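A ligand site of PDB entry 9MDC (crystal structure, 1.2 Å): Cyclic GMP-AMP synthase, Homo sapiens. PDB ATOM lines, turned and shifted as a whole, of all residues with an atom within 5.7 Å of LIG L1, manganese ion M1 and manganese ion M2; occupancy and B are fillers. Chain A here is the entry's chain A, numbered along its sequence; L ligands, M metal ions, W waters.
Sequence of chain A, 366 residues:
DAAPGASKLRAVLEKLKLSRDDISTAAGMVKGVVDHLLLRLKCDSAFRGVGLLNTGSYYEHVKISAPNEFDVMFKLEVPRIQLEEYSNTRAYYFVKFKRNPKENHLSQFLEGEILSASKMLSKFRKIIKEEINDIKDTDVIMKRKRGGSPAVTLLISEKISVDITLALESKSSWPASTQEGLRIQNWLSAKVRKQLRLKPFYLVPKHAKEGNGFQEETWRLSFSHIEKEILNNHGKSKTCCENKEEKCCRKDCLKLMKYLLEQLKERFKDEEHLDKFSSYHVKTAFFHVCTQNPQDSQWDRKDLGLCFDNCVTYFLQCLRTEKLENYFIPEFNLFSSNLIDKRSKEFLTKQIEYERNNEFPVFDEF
Of the 20 residues printed, 3 come within 4 Å of manganese ion M1.
The nearest printed residue that does not touch manganese ion M1 is Phe 70 (4.8 Å).
Ser 149 touches LIG L1.
CG of Pro 150 touches C15 of LIG L1, at 3.7 Å.
CB of Ala 151 touches C11 of LIG L1 (3.6 Å).
Thr 165 touches LIG L1.
Val 204 touches LIG L1.
CD of Lys 206 touches CL2 of LIG L1, 3.1 Å away.
CZ of Arg 220 touches CL2 of LIG L1, at 3.2 Å.
Leu 221 touches LIG L1 (O to CL1, 3.1 Å).
Ser 222 touches LIG L1.
Hydrophobic or aromatic side chains that line LIG L1: Pro 150, Ala 151 and Val 204.
The nearest printed residue that does not touch LIG L1 is Gly 148 (4.4 Å).
O3 of LG2 L2 is in hydrogen-bond range of OG of Ser 57, 2.6 Å away.
An oxygen (O5) of LG2 L2 lies close to the backbone NH of Ser 57, at 2.9 Å.
N of Lys 63 lies within hydrogen-bond range of O of Ser 57 (3.2 Å).
The backbone NH (N) of Ala 151 lies within hydrogen-bond range of the side-chain hydroxyl (OG) of Ser 149, at 3.1 Å.
The backbone NH (N) of Asp 163 sits at hydrogen-bond distance from the backbone carbonyl oxygen (O) of Phe 70 (2.9 Å).
NH1 of Arg 220 lies within hydrogen-bond range of OH of Tyr 92, 2.8 Å away.
O of Arg 220 is in hydrogen-bond range of N of Val 204.
NZ of Lys 206 lies within hydrogen-bond range of O of Gly 148.
Manganese ion M2 is bound by OE1 of Glu 69 (2.1 Å), O2 of LG2 L2 (2.1 Å), O5 of LG2 L2 (2.1 Å), OD2 of Asp 71 (2.2 Å), O7 of LG2 L2 (2.2 Å) and water W5 (2.3 Å).
Manganese ion M2 has six donor atoms within binding distance.
Water W5 lies within hydrogen-bond range of OG of Ser 57 (2.7 Å) and O of Glu 69 (2.9 Å).
Residues that only touch manganese ion M2: Ser 57 (3.96 Å).
Within 4 Å of manganese ion M2: Ser 57, Glu 69 and Asp 71.
Manganese ion M1 is bound by the side-chain carboxylate of Glu 69, the side-chain carboxylate of Asp 163, the side-chain carboxylate of Asp 71, an oxygen (O1) of LIG L1, an oxygen (O7) of LG2 L2 and a nitrogen (N3) of LIG L1.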
ATOM      1  N   GLY A  56       8.619  -4.473  -4.733  1.00  0.00           N
ATOM      2  CA  GLY A  56       8.022  -3.861  -5.895  1.00  0.00           C
ATOM      3  C   GLY A  56       9.027  -3.306  -6.884  1.00  0.00           C
ATOM      4  O   GLY A  56      10.258  -3.445  -6.751  1.00  0.00           O
ATOM      5  N   SER A  57       8.486  -2.624  -7.902  1.00  0.00           N
ATOM      6  CA  SER A  57       9.259  -2.419  -9.127  1.00  0.00           C
ATOM      7  C   SER A  57      10.461  -1.505  -8.940  1.00  0.00           C
ATOM      8  O   SER A  57      11.454  -1.660  -9.647  1.00  0.00           O
ATOM      9  CB  SER A  57       8.379  -1.881 -10.250  1.00  0.00           C
ATOM     10  OG  SER A  57       7.885  -0.591  -9.925  1.00  0.00           O
ATOM     11  N   TYR A  58      10.392  -0.516  -8.034  1.00  0.00           N
ATOM     12  CA  TYR A  58      11.540   0.375  -7.874  1.00  0.00           C
ATOM     13  C   TYR A  58      12.743  -0.424  -7.411  1.00  0.00           C
ATOM     14  O   TYR A  58      13.858  -0.254  -7.932  1.00  0.00           O
ATOM     15  CB  TYR A  58      11.201   1.486  -6.884  1.00  0.00           C
ATOM     16  CG  TYR A  58      12.335   2.437  -6.635  1.00  0.00           C
ATOM     17  CD1 TYR A  58      12.519   3.563  -7.437  1.00  0.00           C
ATOM     18  CD2 TYR A  58      13.231   2.223  -5.598  1.00  0.00           C
ATOM     19  CE1 TYR A  58      13.563   4.449  -7.204  1.00  0.00           C
ATOM     20  CE2 TYR A  58      14.274   3.101  -5.353  1.00  0.00           C
ATOM     21  CZ  TYR A  58      14.430   4.213  -6.158  1.00  0.00           C
ATOM     22  OH  TYR A  58      15.443   5.096  -5.920  1.00  0.00           O
ATOM     23  N   LYS A  63      10.877  -0.274 -12.458  1.00  0.00           N
ATOM     24  CA  LYS A  63      10.007   0.898 -12.459  1.00  0.00           C
ATOM     25  C   LYS A  63      10.245   1.692 -13.733  1.00  0.00           C
ATOM     26  O   LYS A  63      11.392   1.906 -14.130  1.00  0.00           O
ATOM     27  CB  LYS A  63      10.302   1.755 -11.230  1.00  0.00           C
ATOM     28  CG  LYS A  63       9.460   3.008 -11.117  1.00  0.00           C
ATOM     29  CD  LYS A  63       8.085   2.683 -10.557  1.00  0.00           C
ATOM     30  CE  LYS A  63       7.125   3.878 -10.592  1.00  0.00           C
ATOM     31  NZ  LYS A  63       6.723   4.239 -11.994  1.00  0.00           N
ATOM     32  N   GLU A  69       6.392   5.864  -7.521  1.00  0.00           N
ATOM     33  CA  GLU A  69       5.582   4.886  -6.799  1.00  0.00           C
ATOM     34  C   GLU A  69       6.508   3.843  -6.187  1.00  0.00           C
ATOM     35  O   GLU A  69       7.265   3.172  -6.910  1.00  0.00           O
ATOM     36  CB  GLU A  69       4.502   4.249  -7.677  1.00  0.00           C
ATOM     37  CG  GLU A  69       3.307   3.679  -6.881  1.00  0.00           C
ATOM     38  CD  GLU A  69       3.455   2.233  -6.506  1.00  0.00           C
ATOM     39  OE1 GLU A  69       4.462   1.592  -6.868  1.00  0.00           O
ATOM     40  OE2 GLU A  69       2.505   1.726  -5.870  1.00  0.00           O
ATOM     41  N   PHE A  70       6.462   3.743  -4.862  1.00  0.00           N
ATOM     42  CA  PHE A  70       7.339   2.889  -4.081  1.00  0.00           C
ATOM     43  C   PHE A  70       6.486   1.969  -3.224  1.00  0.00           C
ATOM     44  O   PHE A  70       5.424   2.355  -2.736  1.00  0.00           O
ATOM     45  CB  PHE A  70       8.199   3.709  -3.111  1.00  0.00           C
ATOM     46  CG  PHE A  70       9.243   4.570  -3.780  1.00  0.00           C
ATOM     47  CD1 PHE A  70       8.891   5.741  -4.433  1.00  0.00           C
ATOM     48  CD2 PHE A  70      10.587   4.214  -3.746  1.00  0.00           C
ATOM     49  CE1 PHE A  70       9.852   6.535  -5.043  1.00  0.00           C
ATOM     50  CE2 PHE A  70      11.552   5.025  -4.327  1.00  0.00           C
ATOM     51  CZ  PHE A  70      11.181   6.184  -4.982  1.00  0.00           C
ATOM     52  N   ASP A  71       7.007   0.766  -2.966  1.00  0.00           N
ATOM     53  CA  ASP A  71       6.325  -0.225  -2.142  1.00  0.00           C
ATOM     54  C   ASP A  71       7.251  -0.700  -1.043  1.00  0.00           C
ATOM     55  O   ASP A  71       8.400  -1.071  -1.287  1.00  0.00           O
ATOM     56  CB  ASP A  71       5.889  -1.411  -2.987  1.00  0.00           C
ATOM     57  CG  ASP A  71       5.077  -0.983  -4.166  1.00  0.00           C
ATOM     58  OD1 ASP A  71       3.883  -0.686  -3.948  1.00  0.00           O
ATOM     59  OD2 ASP A  71       5.622  -0.946  -5.290  1.00  0.00           O
ATOM     60  N   TYR A  92      -5.478 -17.536   1.543  1.00  0.00           N
ATOM     61  CA  TYR A  92      -5.965 -16.793   2.704  1.00  0.00           C
ATOM     62  C   TYR A  92      -5.996 -17.677   3.936  1.00  0.00           C
ATOM     63  O   TYR A  92      -6.343 -18.861   3.860  1.00  0.00           O
ATOM     64  CB  TYR A  92      -7.353 -16.226   2.449  1.00  0.00           C
ATOM     65  CG  TYR A  92      -7.410 -15.196   1.356  1.00  0.00           C
ATOM     66  CD1 TYR A  92      -7.144 -13.851   1.631  1.00  0.00           C
ATOM     67  CD2 TYR A  92      -7.719 -15.546   0.049  1.00  0.00           C
ATOM     68  CE1 TYR A  92      -7.195 -12.902   0.629  1.00  0.00           C
ATOM     69  CE2 TYR A  92      -7.768 -14.607  -0.950  1.00  0.00           C
ATOM     70  CZ  TYR A  92      -7.514 -13.279  -0.653  1.00  0.00           C
ATOM     71  OH  TYR A  92      -7.557 -12.327  -1.643  1.00  0.00           O
ATOM     72  N   ARG A 146      -8.305   2.138  -0.476  1.00  0.00           N
ATOM     73  CA  ARG A 146      -8.632   1.448  -1.726  1.00  0.00           C
ATOM     74  C   ARG A 146      -9.052   0.028  -1.361  1.00  0.00           C
ATOM     75  O   ARG A 146      -8.218  -0.765  -0.915  1.00  0.00           O
ATOM     76  CB  ARG A 146      -7.426   1.439  -2.659  1.00  0.00           C
ATOM     77  CG  ARG A 146      -7.154   2.752  -3.366  1.00  0.00           C
ATOM     78  CD  ARG A 146      -8.226   3.039  -4.403  1.00  0.00           C
ATOM     79  NE  ARG A 146      -8.646   1.821  -5.082  1.00  0.00           N
ATOM     80  CZ  ARG A 146      -8.009   1.265  -6.094  1.00  0.00           C
ATOM     81  NH1 ARG A 146      -6.902   1.800  -6.598  1.00  0.00           N
ATOM     82  NH2 ARG A 146      -8.479   0.137  -6.625  1.00  0.00           N
ATOM     83  N   GLY A 148      -9.687  -3.730  -1.043  1.00  0.00           N
ATOM     84  CA  GLY A 148      -8.841  -4.823  -1.491  1.00  0.00           C
ATOM     85  C   GLY A 148      -7.351  -4.567  -1.428  1.00  0.00           C
ATOM     86  O   GLY A 148      -6.575  -5.436  -1.855  1.00  0.00           O
ATOM     87  N   SER A 149      -6.922  -3.409  -0.923  1.00  0.00           N
ATOM     88  CA  SER A 149      -5.469  -3.280  -0.768  1.00  0.00           C
ATOM     89  C   SER A 149      -5.087  -3.507   0.685  1.00  0.00           C
ATOM     90  O   SER A 149      -5.774  -3.034   1.588  1.00  0.00           O
ATOM     91  CB  SER A 149      -5.018  -1.877  -1.175  1.00  0.00           C
ATOM     92  OG  SER A 149      -3.638  -1.695  -0.891  1.00  0.00           O
ATOM     93  N   PRO A 150      -3.998  -4.247   0.923  1.00  0.00           N
ATOM     94  CA  PRO A 150      -3.493  -4.385   2.300  1.00  0.00           C
ATOM     95  C   PRO A 150      -2.643  -3.207   2.734  1.00  0.00           C
ATOM     96  O   PRO A 150      -2.182  -3.196   3.883  1.00  0.00           O
ATOM     97  CB  PRO A 150      -2.650  -5.666   2.203  1.00  0.00           C
ATOM     98  CG  PRO A 150      -2.099  -5.619   0.807  1.00  0.00           C
ATOM     99  CD  PRO A 150      -3.210  -5.033  -0.040  1.00  0.00           C
ATOM    100  N   ALA A 151      -2.415  -2.225   1.867  1.00  0.00           N
ATOM    101  CA  ALA A 151      -1.478  -1.148   2.132  1.00  0.00           C
ATOM    102  C   ALA A 151      -2.166   0.111   2.641  1.00  0.00           C
ATOM    103  O   ALA A 151      -3.340   0.379   2.369  1.00  0.00           O
ATOM    104  CB  ALA A 151      -0.700  -0.797   0.866  1.00  0.00           C
ATOM    105  N   ASP A 163       3.283   2.884  -0.930  1.00  0.00           N
ATOM    106  CA  ASP A 163       2.426   1.866  -0.314  1.00  0.00           C
ATOM    107  C   ASP A 163       3.173   1.219   0.845  1.00  0.00           C
ATOM    108  O   ASP A 163       4.226   0.629   0.638  1.00  0.00           O
ATOM    109  CB  ASP A 163       2.047   0.806  -1.351  1.00  0.00           C
ATOM    110  CG  ASP A 163       1.100   1.317  -2.419  1.00  0.00           C
ATOM    111  OD1 ASP A 163       0.402   2.323  -2.151  1.00  0.00           O
ATOM    112  OD2 ASP A 163       1.057   0.719  -3.503  1.00  0.00           O
ATOM    113  N   THR A 165       2.781  -1.670   3.536  1.00  0.00           N
ATOM    114  CA  THR A 165       2.005  -2.870   3.863  1.00  0.00           C
ATOM    115  C   THR A 165       2.495  -3.483   5.159  1.00  0.00           C
ATOM    116  O   THR A 165       3.647  -3.929   5.255  1.00  0.00           O
ATOM    117  CB  THR A 165       2.069  -3.892   2.724  1.00  0.00           C
ATOM    118  OG1 THR A 165       1.534  -3.312   1.530  1.00  0.00           O
ATOM    119  CG2 THR A 165       1.240  -5.113   3.076  1.00  0.00           C
ATOM    120  N   VAL A 204      -0.191 -10.636   4.899  1.00  0.00           N
ATOM    121  CA  VAL A 204      -0.587  -9.236   4.804  1.00  0.00           C
ATOM    122  C   VAL A 204      -2.099  -9.124   5.004  1.00  0.00           C
ATOM    123  O   VAL A 204      -2.835 -10.088   4.727  1.00  0.00           O
ATOM    124  CB  VAL A 204      -0.119  -8.604   3.477  1.00  0.00           C
ATOM    125  CG1 VAL A 204       1.389  -8.755   3.337  1.00  0.00           C
ATOM    126  CG2 VAL A 204      -0.836  -9.224   2.277  1.00  0.00           C
ATOM    127  N   LYS A 206      -4.867  -8.446   3.631  1.00  0.00           N
ATOM    128  CA  LYS A 206      -5.821  -8.459   2.536  1.00  0.00           C
ATOM    129  C   LYS A 206      -6.791  -9.593   2.797  1.00  0.00           C
ATOM    130  O   LYS A 206      -6.368 -10.742   2.981  1.00  0.00           O
ATOM    131  CB  LYS A 206      -5.128  -8.663   1.191  1.00  0.00           C
ATOM    132  CG  LYS A 206      -6.122  -8.752   0.050  1.00  0.00           C
ATOM    133  CD  LYS A 206      -5.477  -8.705  -1.304  1.00  0.00           C
ATOM    134  CE  LYS A 206      -6.505  -8.973  -2.394  1.00  0.00           C
ATOM    135  NZ  LYS A 206      -7.713  -8.114  -2.244  1.00  0.00           N
ATOM    136  N   ARG A 220      -3.497 -12.733   3.941  1.00  0.00           N
ATOM    137  CA  ARG A 220      -3.116 -13.336   2.676  1.00  0.00           C
ATOM    138  C   ARG A 220      -1.603 -13.541   2.611  1.00  0.00           C
ATOM    139  O   ARG A 220      -0.818 -12.686   3.057  1.00  0.00           O
ATOM    140  CB  ARG A 220      -3.553 -12.472   1.496  1.00  0.00           C
ATOM    141  CG  ARG A 220      -3.247 -13.101   0.158  1.00  0.00           C
ATOM    142  CD  ARG A 220      -4.069 -12.508  -0.932  1.00  0.00           C
ATOM    143  NE  ARG A 220      -3.580 -12.884  -2.252  1.00  0.00           N
ATOM    144  CZ  ARG A 220      -4.196 -12.578  -3.385  1.00  0.00           C
ATOM    145  NH1 ARG A 220      -5.386 -12.000  -3.382  1.00  0.00           N
ATOM    146  NH2 ARG A 220      -3.591 -12.830  -4.540  1.00  0.00           N
ATOM    147  N   LEU A 221      -1.172 -14.676   2.052  1.00  0.00           N
ATOM    148  CA  LEU A 221       0.244 -14.936   1.884  1.00  0.00           C
ATOM    149  C   LEU A 221       0.878 -13.942   0.923  1.00  0.00           C
ATOM    150  O   LEU A 221       0.285 -13.576  -0.102  1.00  0.00           O
ATOM    151  CB  LEU A 221       0.478 -16.348   1.342  1.00  0.00           C
ATOM    152  CG  LEU A 221       0.111 -17.533   2.243  1.00  0.00           C
ATOM    153  CD1 LEU A 221       0.304 -18.843   1.493  1.00  0.00           C
ATOM    154  CD2 LEU A 221       0.945 -17.500   3.528  1.00  0.00           C
ATOM    155  N   SER A 222       2.103 -13.514   1.228  1.00  0.00           N
ATOM    156  CA  SER A 222       2.869 -12.691   0.310  1.00  0.00           C
ATOM    157  C   SER A 222       4.284 -13.215   0.207  1.00  0.00           C
ATOM    158  O   SER A 222       4.936 -13.492   1.227  1.00  0.00           O
ATOM    159  CB  SER A 222       2.891 -11.230   0.760  1.00  0.00           C
ATOM    160  OG  SER A 222       3.663 -10.465  -0.145  1.00  0.00           O
HETATM  161  C1  LIG L   1       0.481  -8.165  -1.360  1.00  0.00           C
HETATM  162  C2  LIG L   1      -2.424  -2.943  -4.129  1.00  0.00           C
HETATM  163  C3  LIG L   1      -0.313  -3.846  -3.140  1.00  0.00           C
HETATM  164  C4  LIG L   1      -0.164  -2.108  -4.797  1.00  0.00           C
HETATM  165  C5  LIG L   1      -0.645  -1.254  -5.953  1.00  0.00           C
HETATM  166  C6  LIG L   1      -0.273   0.578  -7.270  1.00  0.00           C
HETATM  167  C7  LIG L   1      -1.387   0.285  -8.028  1.00  0.00           C
HETATM  168  C8  LIG L   1      -2.082  -0.860  -7.685  1.00  0.00           C
HETATM  169  C9  LIG L   1      -0.830   1.912  -9.742  1.00  0.00           C
HETATM  170  C10 LIG L   1      -1.519   2.541 -10.916  1.00  0.00           C
HETATM  171  C11 LIG L   1      -0.177  -3.173  -1.781  1.00  0.00           C
HETATM  172  C12 LIG L   1      -0.525  -9.066  -1.676  1.00  0.00           C
HETATM  173  C13 LIG L   1      -1.636  -8.635  -2.386  1.00  0.00           C
HETATM  174  C14 LIG L   1      -1.713  -7.318  -2.814  1.00  0.00           C
HETATM  175  C15 LIG L   1      -0.675  -6.407  -2.514  1.00  0.00           C
HETATM  176  C16 LIG L   1       0.432  -6.841  -1.772  1.00  0.00           C
HETATM  177  C17 LIG L   1      -2.249  -5.347  -3.715  1.00  0.00           C
HETATM  178  C18 LIG L   1      -1.054  -5.149  -3.097  1.00  0.00           C
HETATM  179  C19 LIG L   1      -2.999  -4.312  -4.496  1.00  0.00           C
HETATM  180  N1  LIG L   1      -2.664  -6.645  -3.541  1.00  0.00           N
HETATM  181  N2  LIG L   1      -0.969  -2.947  -4.103  1.00  0.00           N
HETATM  182  N3  LIG L   1       0.093  -0.184  -6.240  1.00  0.00           N
HETATM  183  N4  LIG L   1      -1.713  -1.634  -6.662  1.00  0.00           N
HETATM  184  O1  LIG L   1       1.030  -1.970  -4.522  1.00  0.00           O
HETATM  185  O2  LIG L   1      -1.778   1.056  -9.096  1.00  0.00           O
HETATM  186  O3  LIG L   1      -2.710   3.192 -10.511  1.00  0.00           O
HETATM  187 CL1  LIG L   1      -0.389 -10.729  -1.164  1.00  0.00          CL
HETATM  188 CL2  LIG L   1      -2.925  -9.707  -2.810  1.00  0.00          CL
HETATM  189  P1  LG2 L   2       4.542  -0.811 -10.699  1.00  0.00           P
HETATM  190  O1  LG2 L   2       3.272  -0.791 -11.545  1.00  0.00           O
HETATM  191  O2  LG2 L   2       4.397  -0.179  -9.339  1.00  0.00           O
HETATM  192  O3  LG2 L   2       5.762  -0.357 -11.476  1.00  0.00           O
HETATM  193  P2  LG2 L   2       4.889  -3.204  -8.947  1.00  0.00           P
HETATM  194  O4  LG2 L   2       5.265  -4.628  -9.123  1.00  0.00           O
HETATM  195  O5  LG2 L   2       5.616  -2.369  -7.935  1.00  0.00           O
HETATM  196  N1  LG2 L   2       4.879  -2.505 -10.420  1.00  0.00           N
HETATM  197  P3  LG2 L   2       2.435  -2.710  -7.315  1.00  0.00           P
HETATM  198  O6  LG2 L   2       1.022  -2.749  -7.772  1.00  0.00           O
HETATM  199  O7  LG2 L   2       2.988  -1.404  -6.772  1.00  0.00           O
HETATM  200  O8  LG2 L   2       3.288  -3.236  -8.527  1.00  0.00           O
HETATM  201  O9  LG2 L   2       2.607  -3.873  -6.232  1.00  0.00           O
HETATM  202  C1  LG2 L   2       3.766  -3.935  -5.421  1.00  0.00           C
HETATM  203  C2  LG2 L   2       4.081  -5.388  -5.114  1.00  0.00           C
HETATM  204  O10 LG2 L   2       2.995  -5.962  -4.346  1.00  0.00           O
HETATM  205  C3  LG2 L   2       4.185  -6.337  -6.312  1.00  0.00           C
HETATM  206  O11 LG2 L   2       5.411  -6.250  -6.979  1.00  0.00           O
HETATM  207  C4  LG2 L   2       3.859  -7.674  -5.684  1.00  0.00           C
HETATM  208  O12 LG2 L   2       5.038  -8.198  -5.096  1.00  0.00           O
HETATM  209  C5  LG2 L   2       2.789  -7.300  -4.621  1.00  0.00           C
HETATM  210  N2  LG2 L   2       1.455  -7.476  -5.169  1.00  0.00           N
HETATM  211  C6  LG2 L   2       0.666  -6.577  -5.847  1.00  0.00           C
HETATM  212  N3  LG2 L   2      -0.468  -7.079  -6.252  1.00  0.00           N
HETATM  213  C7  LG2 L   2      -0.434  -8.381  -5.827  1.00  0.00           C
HETATM  214  C8  LG2 L   2      -1.336  -9.460  -5.938  1.00  0.00           C
HETATM  215  N4  LG2 L   2      -2.525  -9.358  -6.564  1.00  0.00           N
HETATM  216  N5  LG2 L   2      -0.980 -10.631  -5.419  1.00  0.00           N
HETATM  217  C9  LG2 L   2       0.192 -10.747  -4.803  1.00  0.00           C
HETATM  218  N6  LG2 L   2       1.108  -9.819  -4.637  1.00  0.00           N
HETATM  219  C10 LG2 L   2       0.753  -8.650  -5.165  1.00  0.00           C
HETATM  220 MN    MN M   1       2.140  -0.199  -5.085  1.00  0.00          MN
HETATM  221 MN    MN M   2       4.925  -0.439  -7.295  1.00  0.00          MN
HETATM  222  O   HOH W   1      -3.822  -3.604  -7.927  1.00  0.00           O
HETATM  223  O   HOH W   2       2.321   1.693  -9.470  1.00  0.00           O
HETATM  224  O   HOH W   3       0.847  -1.091 -10.190  1.00  0.00           O
HETATM  225  O   HOH W   4      -5.126  -7.323  -5.160  1.00  0.00           O
HETATM  226  O   HOH W   5       7.001   0.396  -7.564  1.00  0.00           O
